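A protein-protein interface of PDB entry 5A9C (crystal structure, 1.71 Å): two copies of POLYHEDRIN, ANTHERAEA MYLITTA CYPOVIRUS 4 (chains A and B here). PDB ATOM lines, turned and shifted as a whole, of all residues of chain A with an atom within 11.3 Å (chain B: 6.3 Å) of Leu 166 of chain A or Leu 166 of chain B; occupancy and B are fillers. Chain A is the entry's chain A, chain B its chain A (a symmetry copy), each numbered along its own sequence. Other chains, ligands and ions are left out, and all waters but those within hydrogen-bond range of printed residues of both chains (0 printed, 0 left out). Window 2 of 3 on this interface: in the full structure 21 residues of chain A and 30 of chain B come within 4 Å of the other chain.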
ATOM      1  N   GLN A  34      11.550 -24.731   5.581  1.00  0.00           N
ATOM      2  CA  GLN A  34      12.002 -24.914   4.198  1.00  0.00           C
ATOM      3  C   GLN A  34      12.355 -23.638   3.423  1.00  0.00           C
ATOM      4  O   GLN A  34      13.219 -23.667   2.548  1.00  0.00           O
ATOM      5  CB  GLN A  34      10.996 -25.759   3.413  1.00  0.00           C
ATOM      6  CG  GLN A  34      10.978 -27.220   3.838  1.00  0.00           C
ATOM      7  CD  GLN A  34       9.862 -28.003   3.182  1.00  0.00           C
ATOM      8  OE1 GLN A  34       9.183 -27.506   2.283  1.00  0.00           O
ATOM      9  NE2 GLN A  34       9.661 -29.237   3.633  1.00  0.00           N
ATOM     10  N   PRO A  59      18.086 -18.300   0.615  1.00  0.00           N
ATOM     11  CA  PRO A  59      17.159 -19.318   1.126  1.00  0.00           C
ATOM     12  C   PRO A  59      17.455 -20.770   0.733  1.00  0.00           C
ATOM     13  O   PRO A  59      17.031 -21.670   1.459  1.00  0.00           O
ATOM     14  CB  PRO A  59      15.821 -18.890   0.524  1.00  0.00           C
ATOM     15  CG  PRO A  59      16.199 -18.259  -0.771  1.00  0.00           C
ATOM     16  CD  PRO A  59      17.517 -17.555  -0.522  1.00  0.00           C
ATOM     17  N   ASP A  60      18.151 -21.004  -0.375  1.00  0.00           N
ATOM     18  CA  ASP A  60      18.285 -22.372  -0.883  1.00  0.00           C
ATOM     19  C   ASP A  60      19.720 -22.837  -1.120  1.00  0.00           C
ATOM     20  O   ASP A  60      20.114 -23.913  -0.664  1.00  0.00           O
ATOM     21  CB  ASP A  60      17.461 -22.545  -2.160  1.00  0.00           C
ATOM     22  CG  ASP A  60      15.973 -22.415  -1.908  1.00  0.00           C
ATOM     23  OD1 ASP A  60      15.443 -23.182  -1.077  1.00  0.00           O
ATOM     24  OD2 ASP A  60      15.337 -21.547  -2.541  1.00  0.00           O
ATOM     25  N   TYR A  61      20.495 -22.040  -1.847  1.00  0.00           N
ATOM     26  CA  TYR A  61      21.878 -22.399  -2.131  1.00  0.00           C
ATOM     27  C   TYR A  61      22.715 -21.173  -2.456  1.00  0.00           C
ATOM     28  O   TYR A  61      22.202 -20.146  -2.905  1.00  0.00           O
ATOM     29  CB  TYR A  61      21.959 -23.411  -3.280  1.00  0.00           C
ATOM     30  CG  TYR A  61      21.411 -22.886  -4.586  1.00  0.00           C
ATOM     31  CD1 TYR A  61      22.228 -22.209  -5.484  1.00  0.00           C
ATOM     32  CD2 TYR A  61      20.073 -23.055  -4.916  1.00  0.00           C
ATOM     33  CE1 TYR A  61      21.726 -21.718  -6.675  1.00  0.00           C
ATOM     34  CE2 TYR A  61      19.563 -22.568  -6.105  1.00  0.00           C
ATOM     35  CZ  TYR A  61      20.393 -21.899  -6.979  1.00  0.00           C
ATOM     36  OH  TYR A  61      19.886 -21.415  -8.165  1.00  0.00           O
ATOM     37  N   LYS A  63      26.490 -20.159  -4.344  1.00  0.00           N
ATOM     38  CA  LYS A  63      27.736 -20.427  -5.049  1.00  0.00           C
ATOM     39  C   LYS A  63      28.539 -19.136  -5.126  1.00  0.00           C
ATOM     40  O   LYS A  63      28.085 -18.152  -5.710  1.00  0.00           O
ATOM     41  CB  LYS A  63      27.457 -20.954  -6.460  1.00  0.00           C
ATOM     42  CG  LYS A  63      26.692 -22.264  -6.496  1.00  0.00           C
ATOM     43  CD  LYS A  63      26.332 -22.649  -7.923  1.00  0.00           C
ATOM     44  CE  LYS A  63      25.527 -21.548  -8.597  1.00  0.00           C
ATOM     45  NZ  LYS A  63      25.147 -21.903  -9.989  1.00  0.00           N
ATOM     46  N   LEU A 149      30.675 -23.098  -1.423  1.00  0.00           N
ATOM     47  CA  LEU A 149      29.393 -23.721  -1.726  1.00  0.00           C
ATOM     48  C   LEU A 149      28.646 -24.063  -0.443  1.00  0.00           C
ATOM     49  O   LEU A 149      29.189 -24.712   0.449  1.00  0.00           O
ATOM     50  CB  LEU A 149      29.584 -24.993  -2.550  1.00  0.00           C
ATOM     51  CG  LEU A 149      28.315 -25.834  -2.727  1.00  0.00           C
ATOM     52  CD1 LEU A 149      27.272 -25.077  -3.531  1.00  0.00           C
ATOM     53  CD2 LEU A 149      28.629 -27.166  -3.385  1.00  0.00           C
ATOM     54  N   THR A 151      24.565 -25.390   0.698  1.00  0.00           N
ATOM     55  CA  THR A 151      23.235 -25.782   0.252  1.00  0.00           C
ATOM     56  C   THR A 151      22.333 -26.136   1.425  1.00  0.00           C
ATOM     57  O   THR A 151      22.798 -26.637   2.451  1.00  0.00           O
ATOM     58  CB  THR A 151      23.290 -26.977  -0.722  1.00  0.00           C
ATOM     59  OG1 THR A 151      24.016 -28.055  -0.119  1.00  0.00           O
ATOM     60  CG2 THR A 151      23.979 -26.577  -2.020  1.00  0.00           C
ATOM     61  N   ALA A 152      21.040 -25.869   1.263  1.00  0.00           N
ATOM     62  CA  ALA A 152      20.054 -26.184   2.287  1.00  0.00           C
ATOM     63  C   ALA A 152      19.960 -27.689   2.482  1.00  0.00           C
ATOM     64  O   ALA A 152      19.961 -28.451   1.514  1.00  0.00           O
ATOM     65  CB  ALA A 152      18.697 -25.615   1.906  1.00  0.00           C
ATOM     66  N   ASN A 159      12.802 -33.416  -1.079  1.00  0.00           N
ATOM     67  CA  ASN A 159      13.952 -32.538  -1.252  1.00  0.00           C
ATOM     68  C   ASN A 159      13.645 -31.384  -2.201  1.00  0.00           C
ATOM     69  O   ASN A 159      13.056 -31.583  -3.264  1.00  0.00           O
ATOM     70  CB  ASN A 159      15.156 -33.332  -1.763  1.00  0.00           C
ATOM     71  CG  ASN A 159      16.453 -32.554  -1.664  1.00  0.00           C
ATOM     72  OD1 ASN A 159      16.449 -31.335  -1.497  1.00  0.00           O
ATOM     73  ND2 ASN A 159      17.574 -33.258  -1.768  1.00  0.00           N
ATOM     74  N   ARG A 160      14.048 -30.178  -1.813  1.00  0.00           N
ATOM     75  CA  ARG A 160      13.784 -28.985  -2.614  1.00  0.00           C
ATOM     76  C   ARG A 160      14.551 -29.005  -3.933  1.00  0.00           C
ATOM     77  O   ARG A 160      14.321 -28.171  -4.808  1.00  0.00           O
ATOM     78  CB  ARG A 160      14.125 -27.719  -1.822  1.00  0.00           C
ATOM     79  CG  ARG A 160      15.601 -27.555  -1.505  1.00  0.00           C
ATOM     80  CD  ARG A 160      15.832 -26.366  -0.587  1.00  0.00           C
ATOM     81  NE  ARG A 160      15.343 -26.619   0.766  1.00  0.00           N
ATOM     82  CZ  ARG A 160      15.274 -25.696   1.719  1.00  0.00           C
ATOM     83  NH1 ARG A 160      15.655 -24.450   1.468  1.00  0.00           N
ATOM     84  NH2 ARG A 160      14.819 -26.016   2.923  1.00  0.00           N
ATOM     85  N   PHE A 161      15.465 -29.960  -4.067  1.00  0.00           N
ATOM     86  CA  PHE A 161      16.251 -30.103  -5.287  1.00  0.00           C
ATOM     87  C   PHE A 161      15.736 -31.253  -6.149  1.00  0.00           C
ATOM     88  O   PHE A 161      16.299 -31.551  -7.202  1.00  0.00           O
ATOM     89  CB  PHE A 161      17.730 -30.316  -4.955  1.00  0.00           C
ATOM     90  CG  PHE A 161      18.381 -29.136  -4.286  1.00  0.00           C
ATOM     91  CD1 PHE A 161      18.695 -27.999  -5.012  1.00  0.00           C
ATOM     92  CD2 PHE A 161      18.691 -29.171  -2.937  1.00  0.00           C
ATOM     93  CE1 PHE A 161      19.296 -26.915  -4.404  1.00  0.00           C
ATOM     94  CE2 PHE A 161      19.295 -28.087  -2.321  1.00  0.00           C
ATOM     95  CZ  PHE A 161      19.597 -26.959  -3.056  1.00  0.00           C
ATOM     96  N   ASN A 162      14.664 -31.895  -5.695  1.00  0.00           N
ATOM     97  CA  ASN A 162      14.092 -33.035  -6.409  1.00  0.00           C
ATOM     98  C   ASN A 162      12.905 -32.674  -7.299  1.00  0.00           C
ATOM     99  O   ASN A 162      12.049 -31.875  -6.920  1.00  0.00           O
ATOM    100  CB  ASN A 162      13.676 -34.135  -5.427  1.00  0.00           C
ATOM    101  CG  ASN A 162      14.787 -35.134  -5.164  1.00  0.00           C
ATOM    102  OD1 ASN A 162      15.666 -35.339  -6.002  1.00  0.00           O
ATOM    103  ND2 ASN A 162      14.748 -35.769  -3.998  1.00  0.00           N
ATOM    104  N   GLY A 163      12.873 -33.277  -8.484  1.00  0.00           N
ATOM    105  CA  GLY A 163      11.742 -33.179  -9.390  1.00  0.00           C
ATOM    106  C   GLY A 163      11.061 -31.828  -9.504  1.00  0.00           C
ATOM    107  O   GLY A 163      11.614 -30.895 -10.088  1.00  0.00           O
ATOM    108  N   PRO A 164       9.849 -31.717  -8.939  1.00  0.00           N
ATOM    109  CA  PRO A 164       8.987 -30.544  -9.119  1.00  0.00           C
ATOM    110  C   PRO A 164       9.338 -29.370  -8.205  1.00  0.00           C
ATOM    111  O   PRO A 164       8.961 -28.238  -8.505  1.00  0.00           O
ATOM    112  CB  PRO A 164       7.591 -31.084  -8.787  1.00  0.00           C
ATOM    113  CG  PRO A 164       7.819 -32.326  -7.950  1.00  0.00           C
ATOM    114  CD  PRO A 164       9.286 -32.668  -7.966  1.00  0.00           C
ATOM    115  N   GLN A 165      10.046 -29.634  -7.113  1.00  0.00           N
ATOM    116  CA  GLN A 165      10.425 -28.575  -6.183  1.00  0.00           C
ATOM    117  C   GLN A 165      11.619 -27.768  -6.685  1.00  0.00           C
ATOM    118  O   GLN A 165      11.830 -26.633  -6.261  1.00  0.00           O
ATOM    119  CB  GLN A 165      10.718 -29.147  -4.793  1.00  0.00           C
ATOM    120  CG  GLN A 165       9.491 -29.274  -3.906  1.00  0.00           C
ATOM    121  CD  GLN A 165       8.395 -30.104  -4.541  1.00  0.00           C
ATOM    122  OE1 GLN A 165       8.530 -31.317  -4.695  1.00  0.00           O
ATOM    123  NE2 GLN A 165       7.301 -29.451  -4.918  1.00  0.00           N
ATOM    124  N   LEU A 166      12.393 -28.355  -7.592  1.00  0.00           N
ATOM    125  CA  LEU A 166      13.578 -27.694  -8.126  1.00  0.00           C
ATOM    126  C   LEU A 166      13.224 -26.382  -8.817  1.00  0.00           C
ATOM    127  O   LEU A 166      14.008 -25.433  -8.805  1.00  0.00           O
ATOM    128  CB  LEU A 166      14.322 -28.616  -9.095  1.00  0.00           C
ATOM    129  CG  LEU A 166      15.623 -28.066  -9.683  1.00  0.00           C
ATOM    130  CD1 LEU A 166      16.562 -27.592  -8.582  1.00  0.00           C
ATOM    131  CD2 LEU A 166      16.304 -29.108 -10.559  1.00  0.00           C
ATOM    132  N   ALA A 167      12.037 -26.332  -9.414  1.00  0.00           N
ATOM    133  CA  ALA A 167      11.579 -25.137 -10.113  1.00  0.00           C
ATOM    134  C   ALA A 167      11.432 -23.954  -9.163  1.00  0.00           C
ATOM    135  O   ALA A 167      11.975 -22.878  -9.411  1.00  0.00           O
ATOM    136  CB  ALA A 167      10.267 -25.412 -10.831  1.00  0.00           C
ATOM    137  N   GLN A 168      10.695 -24.155  -8.074  1.00  0.00           N
ATOM    138  CA  GLN A 168      10.496 -23.095  -7.093  1.00  0.00           C
ATOM    139  C   GLN A 168      11.822 -22.686  -6.462  1.00  0.00           C
ATOM    140  O   GLN A 168      12.079 -21.501  -6.256  1.00  0.00           O
ATOM    141  CB  GLN A 168       9.516 -23.534  -6.001  1.00  0.00           C
ATOM    142  CG  GLN A 168       9.301 -22.482  -4.920  1.00  0.00           C
ATOM    143  CD  GLN A 168       8.294 -22.910  -3.867  1.00  0.00           C
ATOM    144  OE1 GLN A 168       8.073 -24.101  -3.647  1.00  0.00           O
ATOM    145  NE2 GLN A 168       7.676 -21.934  -3.212  1.00  0.00           N
ATOM    146  N   THR A 169      12.658 -23.672  -6.159  1.00  0.00           N
ATOM    147  CA  THR A 169      13.962 -23.420  -5.554  1.00  0.00           C
ATOM    148  C   THR A 169      14.814 -22.503  -6.426  1.00  0.00           C
ATOM    149  O   THR A 169      15.462 -21.583  -5.932  1.00  0.00           O
ATOM    150  CB  THR A 169      14.722 -24.736  -5.306  1.00  0.00           C
ATOM    151  OG1 THR A 169      14.049 -25.492  -4.292  1.00  0.00           O
ATOM    152  CG2 THR A 169      16.149 -24.455  -4.861  1.00  0.00           C
ATOM    153  N   LEU A 170      14.808 -22.764  -7.727  1.00  0.00           N
ATOM    154  CA  LEU A 170      15.582 -21.974  -8.676  1.00  0.00           C
ATOM    155  C   LEU A 170      15.120 -20.518  -8.697  1.00  0.00           C
ATOM    156  O   LEU A 170      15.936 -19.596  -8.652  1.00  0.00           O
ATOM    157  CB  LEU A 170      15.486 -22.595 -10.073  1.00  0.00           C
ATOM    158  CG  LEU A 170      16.211 -21.917 -11.238  1.00  0.00           C
ATOM    159  CD1 LEU A 170      15.430 -20.710 -11.720  1.00  0.00           C
ATOM    160  CD2 LEU A 170      17.629 -21.525 -10.842  1.00  0.00           C
ATOM    161  N   THR A 171      13.807 -20.319  -8.759  1.00  0.00           N
ATOM    162  CA  THR A 171      13.233 -18.980  -8.865  1.00  0.00           C
ATOM    163  C   THR A 171      13.127 -18.282  -7.512  1.00  0.00           C
ATOM    164  O   THR A 171      13.046 -17.055  -7.441  1.00  0.00           O
ATOM    165  CB  THR A 171      11.838 -19.026  -9.516  1.00  0.00           C
ATOM    166  OG1 THR A 171      10.953 -19.804  -8.699  1.00  0.00           O
ATOM    167  CG2 THR A 171      11.918 -19.654 -10.896  1.00  0.00           C
ATOM    168  N   ASN A 172      13.131 -19.068  -6.442  1.00  0.00           N
ATOM    169  CA  ASN A 172      12.976 -18.539  -5.090  1.00  0.00           C
ATOM    170  C   ASN A 172      14.300 -18.084  -4.484  1.00  0.00           C
ATOM    171  O   ASN A 172      14.325 -17.315  -3.521  1.00  0.00           O
ATOM    172  CB  ASN A 172      12.336 -19.601  -4.193  1.00  0.00           C
ATOM    173  CG  ASN A 172      12.204 -19.153  -2.756  1.00  0.00           C
ATOM    174  OD1 ASN A 172      13.108 -19.352  -1.946  1.00  0.00           O
ATOM    175  ND2 ASN A 172      11.067 -18.551  -2.427  1.00  0.00           N
ATOM    176  N   ASN A 173      15.399 -18.562  -5.056  1.00  0.00           N
ATOM    177  CA  ASN A 173      16.719 -18.326  -4.480  1.00  0.00           C
ATOM    178  C   ASN A 173      17.369 -17.008  -4.902  1.00  0.00           C
ATOM    179  O   ASN A 173      18.153 -16.965  -5.852  1.00  0.00           O
ATOM    180  CB  ASN A 173      17.648 -19.504  -4.784  1.00  0.00           C
ATOM    181  CG  ASN A 173      18.962 -19.414  -4.038  1.00  0.00           C
ATOM    182  OD1 ASN A 173      19.005 -19.549  -2.815  1.00  0.00           O
ATOM    183  ND2 ASN A 173      20.044 -19.188  -4.772  1.00  0.00           N
ATOM    184  N   ILE A 174      17.043 -15.936  -4.186  1.00  0.00           N
ATOM    185  CA  ILE A 174      17.672 -14.642  -4.416  1.00  0.00           C
ATOM    186  C   ILE A 174      18.788 -14.418  -3.403  1.00  0.00           C
ATOM    187  O   ILE A 174      18.526 -14.180  -2.222  1.00  0.00           O
ATOM    188  CB  ILE A 174      16.654 -13.481  -4.306  1.00  0.00           C
ATOM    189  CG1 ILE A 174      15.587 -13.594  -5.398  1.00  0.00           C
ATOM    190  CG2 ILE A 174      17.364 -12.139  -4.386  1.00  0.00           C
ATOM    191  CD1 ILE A 174      14.570 -12.464  -5.374  1.00  0.00           C
ATOM    192  N   ASN B 159      22.304 -37.623 -18.870  1.00  0.00           N
ATOM    193  CA  ASN B 159      22.582 -36.208 -19.084  1.00  0.00           C
ATOM    194  C   ASN B 159      22.544 -35.422 -17.777  1.00  0.00           C
ATOM    195  O   ASN B 159      21.634 -35.594 -16.965  1.00  0.00           O
ATOM    196  CB  ASN B 159      21.586 -35.615 -20.083  1.00  0.00           C
ATOM    197  CG  ASN B 159      22.007 -34.248 -20.584  1.00  0.00           C
ATOM    198  OD1 ASN B 159      22.868 -33.595 -19.995  1.00  0.00           O
ATOM    199  ND2 ASN B 159      21.398 -33.806 -21.678  1.00  0.00           N
ATOM    200  N   ARG B 160      23.535 -34.558 -17.580  1.00  0.00           N
ATOM    201  CA  ARG B 160      23.635 -33.770 -16.354  1.00  0.00           C
ATOM    202  C   ARG B 160      22.500 -32.756 -16.237  1.00  0.00           C
ATOM    203  O   ARG B 160      22.323 -32.127 -15.194  1.00  0.00           O
ATOM    204  CB  ARG B 160      24.990 -33.058 -16.282  1.00  0.00           C
ATOM    205  CG  ARG B 160      25.200 -31.997 -17.347  1.00  0.00           C
ATOM    206  CD  ARG B 160      26.620 -31.456 -17.303  1.00  0.00           C
ATOM    207  NE  ARG B 160      27.592 -32.437 -17.774  1.00  0.00           N
ATOM    208  CZ  ARG B 160      28.910 -32.284 -17.690  1.00  0.00           C
ATOM    209  NH1 ARG B 160      29.417 -31.187 -17.143  1.00  0.00           N
ATOM    210  NH2 ARG B 160      29.721 -33.228 -18.149  1.00  0.00           N
ATOM    211  N   PHE B 161      21.736 -32.601 -17.313  1.00  0.00           N
ATOM    212  CA  PHE B 161      20.605 -31.681 -17.325  1.00  0.00           C
ATOM    213  C   PHE B 161      19.280 -32.428 -17.183  1.00  0.00           C
ATOM    214  O   PHE B 161      18.210 -31.820 -17.210  1.00  0.00           O
ATOM    215  CB  PHE B 161      20.602 -30.844 -18.606  1.00  0.00           C
ATOM    216  CG  PHE B 161      21.778 -29.914 -18.729  1.00  0.00           C
ATOM    217  CD1 PHE B 161      21.849 -28.763 -17.962  1.00  0.00           C
ATOM    218  CD2 PHE B 161      22.803 -30.184 -19.621  1.00  0.00           C
ATOM    219  CE1 PHE B 161      22.924 -27.904 -18.074  1.00  0.00           C
ATOM    220  CE2 PHE B 161      23.883 -29.325 -19.739  1.00  0.00           C
ATOM    221  CZ  PHE B 161      23.943 -28.185 -18.964  1.00  0.00           C
ATOM    222  N   ASN B 162      19.359 -33.746 -17.031  1.00  0.00           N
ATOM    223  CA  ASN B 162      18.165 -34.579 -16.917  1.00  0.00           C
ATOM    224  C   ASN B 162      17.783 -34.920 -15.479  1.00  0.00           C
ATOM    225  O   ASN B 162      18.643 -35.211 -14.647  1.00  0.00           O
ATOM    226  CB  ASN B 162      18.328 -35.873 -17.721  1.00  0.00           C
ATOM    227  CG  ASN B 162      17.837 -35.740 -19.150  1.00  0.00           C
ATOM    228  OD1 ASN B 162      16.963 -34.924 -19.445  1.00  0.00           O
ATOM    229  ND2 ASN B 162      18.390 -36.553 -20.043  1.00  0.00           N
ATOM    230  N   GLY B 163      16.483 -34.879 -15.205  1.00  0.00           N
ATOM    231  CA  GLY B 163      15.926 -35.327 -13.940  1.00  0.00           C
ATOM    232  C   GLY B 163      16.707 -34.992 -12.683  1.00  0.00           C
ATOM    233  O   GLY B 163      16.747 -33.837 -12.260  1.00  0.00           O
ATOM    234  N   PRO B 164      17.337 -36.011 -12.079  1.00  0.00           N
ATOM    235  CA  PRO B 164      17.977 -35.889 -10.765  1.00  0.00           C
ATOM    236  C   PRO B 164      19.373 -35.268 -10.808  1.00  0.00           C
ATOM    237  O   PRO B 164      19.845 -34.774  -9.785  1.00  0.00           O
ATOM    238  CB  PRO B 164      18.050 -37.341 -10.277  1.00  0.00           C
ATOM    239  CG  PRO B 164      17.953 -38.197 -11.524  1.00  0.00           C
ATOM    240  CD  PRO B 164      17.598 -37.322 -12.697  1.00  0.00           C
ATOM    241  N   GLN B 165      20.018 -35.291 -11.969  1.00  0.00           N
ATOM    242  CA  GLN B 165      21.355 -34.722 -12.102  1.00  0.00           C
ATOM    243  C   GLN B 165      21.324 -33.201 -12.221  1.00  0.00           C
ATOM    244  O   GLN B 165      22.320 -32.531 -11.951  1.00  0.00           O
ATOM    245  CB  GLN B 165      22.093 -35.333 -13.297  1.00  0.00           C
ATOM    246  CG  GLN B 165      22.840 -36.616 -12.971  1.00  0.00           C
ATOM    247  CD  GLN B 165      21.941 -37.678 -12.371  1.00  0.00           C
ATOM    248  OE1 GLN B 165      21.082 -38.236 -13.052  1.00  0.00           O
ATOM    249  NE2 GLN B 165      22.135 -37.961 -11.088  1.00  0.00           N
ATOM    250  N   LEU B 166      20.177 -32.660 -12.622  1.00  0.00           N
ATOM    251  CA  LEU B 166      20.036 -31.220 -12.800  1.00  0.00           C
ATOM    252  C   LEU B 166      20.302 -30.466 -11.502  1.00  0.00           C
ATOM    253  O   LEU B 166      20.804 -29.342 -11.519  1.00  0.00           O
ATOM    254  CB  LEU B 166      18.643 -30.876 -13.333  1.00  0.00           C
ATOM    255  CG  LEU B 166      18.379 -29.396 -13.624  1.00  0.00           C
ATOM    256  CD1 LEU B 166      19.451 -28.821 -14.541  1.00  0.00           C
ATOM    257  CD2 LEU B 166      16.995 -29.201 -14.226  1.00  0.00           C
ATOM    258  N   ALA B 167      19.969 -31.092 -10.378  1.00  0.00           N
ATOM    259  CA  ALA B 167      20.169 -30.480  -9.070  1.00  0.00           C
ATOM    260  C   ALA B 167      21.646 -30.229  -8.789  1.00  0.00           C
ATOM    261  O   ALA B 167      22.040 -29.115  -8.445  1.00  0.00           O
ATOM    262  CB  ALA B 167      19.557 -31.345  -7.978  1.00  0.00           C
ATOM    263  N   GLN B 168      22.463 -31.269  -8.935  1.00  0.00           N
ATOM    264  CA  GLN B 168      23.897 -31.139  -8.702  1.00  0.00           C
ATOM    265  C   GLN B 168      24.518 -30.154  -9.684  1.00  0.00           C
ATOM    266  O   GLN B 168      25.365 -29.345  -9.311  1.00  0.00           O
ATOM    267  CB  GLN B 168      24.597 -32.496  -8.814  1.00  0.00           C
ATOM    268  CG  GLN B 168      26.106 -32.418  -8.624  1.00  0.00           C
ATOM    269  CD  GLN B 168      26.785 -33.775  -8.693  1.00  0.00           C
ATOM    270  OE1 GLN B 168      26.269 -34.711  -9.304  1.00  0.00           O
ATOM    271  NE2 GLN B 168      27.948 -33.886  -8.062  1.00  0.00           N
ATOM    272  N   THR B 169      24.092 -30.228 -10.940  1.00  0.00           N
ATOM    273  CA  THR B 169      24.600 -29.343 -11.982  1.00  0.00           C
ATOM    274  C   THR B 169      24.372 -27.876 -11.629  1.00  0.00           C
ATOM    275  O   THR B 169      25.254 -27.039 -11.806  1.00  0.00           O
ATOM    276  CB  THR B 169      23.940 -29.647 -13.340  1.00  0.00           C
ATOM    277  OG1 THR B 169      24.359 -30.938 -13.797  1.00  0.00           O
ATOM    278  CG2 THR B 169      24.327 -28.597 -14.371  1.00  0.00           C
ATOM    279  N   LEU B 170      23.181 -27.575 -11.128  1.00  0.00           N
ATOM    280  CA  LEU B 170      22.824 -26.212 -10.754  1.00  0.00           C
ATOM    281  C   LEU B 170      23.720 -25.690  -9.633  1.00  0.00           C
ATOM    282  O   LEU B 170      24.230 -24.570  -9.702  1.00  0.00           O
ATOM    283  CB  LEU B 170      21.349 -26.153 -10.343  1.00  0.00           C
ATOM    284  CG  LEU B 170      20.758 -24.817  -9.890  1.00  0.00           C
ATOM    285  CD1 LEU B 170      21.169 -24.509  -8.463  1.00  0.00           C
ATOM    286  CD2 LEU B 170      21.174 -23.692 -10.830  1.00  0.00           C
ATOM    287  N   THR B 171      23.914 -26.509  -8.604  1.00  0.00           N
ATOM    288  CA  THR B 171      24.684 -26.106  -7.430  1.00  0.00           C
ATOM    289  C   THR B 171      26.189 -26.252  -7.641  1.00  0.00           C
ATOM    290  O   THR B 171      26.985 -25.617  -6.949  1.00  0.00           O
ATOM    291  CB  THR B 171      24.270 -26.922  -6.191  1.00  0.00           C
ATOM    292  OG1 THR B 171      24.539 -28.311  -6.419  1.00  0.00           O
ATOM    293  CG2 THR B 171      22.789 -26.744  -5.911  1.00  0.00           C
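The side-chain amino group (NZ) of Lys 63 of chain A lies within hydrogen-bond range of the backbone carbonyl oxygen (O) of Leu 170 of chain B (2.8 Å).
The backbone carbonyl oxygen (O) of Tyr 61 of chain A lies within hydrogen-bond range of the side-chain amide nitrogen (ND2) of Asn 173 of chain A (3.0 Å).
The backbone NH (N) of Phe 161 of chain A sits close to the side-chain amide oxygen (OD1) of Asn 159 of chain A (3.1 Å).
N of Leu 166 of chain A sits at hydrogen-bond distance from O of Arg 160 of chain A (3.4 Å).
O of Arg 160 of chain B lies within hydrogen-bond range of N of Leu 166 of chain B (3.4 Å).
The backbone carbonyl oxygen of Ala 167 of chain B is in hydrogen-bond range of the side-chain hydroxyl of Thr 171 of chain B, 3.3 Å away.
The side-chain hydroxyl (OG1) of Thr 171 of chain B is in hydrogen-bond range of the backbone carbonyl oxygen (O) of Gln 168 of chain B (3.2 Å).
Among the printed residues, merely in contact across the chains: Tyr 61 of chain A with Leu 170 of chain B, Lys 63 of chain A with Thr 171 of chain B, Phe 161 of chain A with Ala 167 of chain B, Leu 149 of chain A with Thr 171 of chain B, Leu 166 of chain A with Leu 166 of chain B and Phe 161 of chain A with Thr 171 of chain B.
Of the printed residues of chain B, Tyr 61 of chain A touches Leu 170.
Of the printed residues of chain B, Phe 161 of chain A touches Ala 167 and Thr 171.
Of the printed residues of chain B, Leu 166 of chain A touches Leu 166 (3.7 Å).
No residue of chain A comes within 4 Å of Phe 161 of chain B.
Gly 163 of chain B touches none of the printed residues of chain A.
Pro 164 of chain B touches none of the printed residues of chain A.
No residue of chain A comes within 4 Å of Gln 165 of chain B.
Leu 166 of chain B touches just one residue of chain A: Leu 166.
Of the printed residues of chain A, Ala 167 of chain B touches Phe 161.
No residue of chain A comes within 4 Å of Thr 169 of chain B.
Of chain A, only Tyr 61 (3.1 Å) and Lys 63 (2.8 Å) come within 4 Å of Leu 170 of chain B.
The nearest residue of chain B that does not touch Leu 166 of chain A is Ala 167 of chain B (4.2 Å).
Of the 13 printed residues of chain B, 4 touch a printed residue of chain A.
Hydrophobic or aromatic side chains of chain B that line the printed part of chain A: Leu 166, Ala 167 and Leu 170.
Along chain B the printed residues that touch a printed residue of chain A span positions 166 to 171.
Among the printed residues, 7 pairs touch across the chains.
Phe 161 of chain A touches Ala 167 of chain B, but with the chains exchanged Ala 167 of chain A does not touch Phe 161 of chain B (11.4 Å).
Phe 161 of chain A touches Thr 171 of chain B, but with the chains exchanged Thr 171 of chain A does not touch Phe 161 of chain B (14.9 Å).
Leu 166 of chain B touches its own counterpart, Leu 166 of chain A.
13 positions are printed for both chains.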
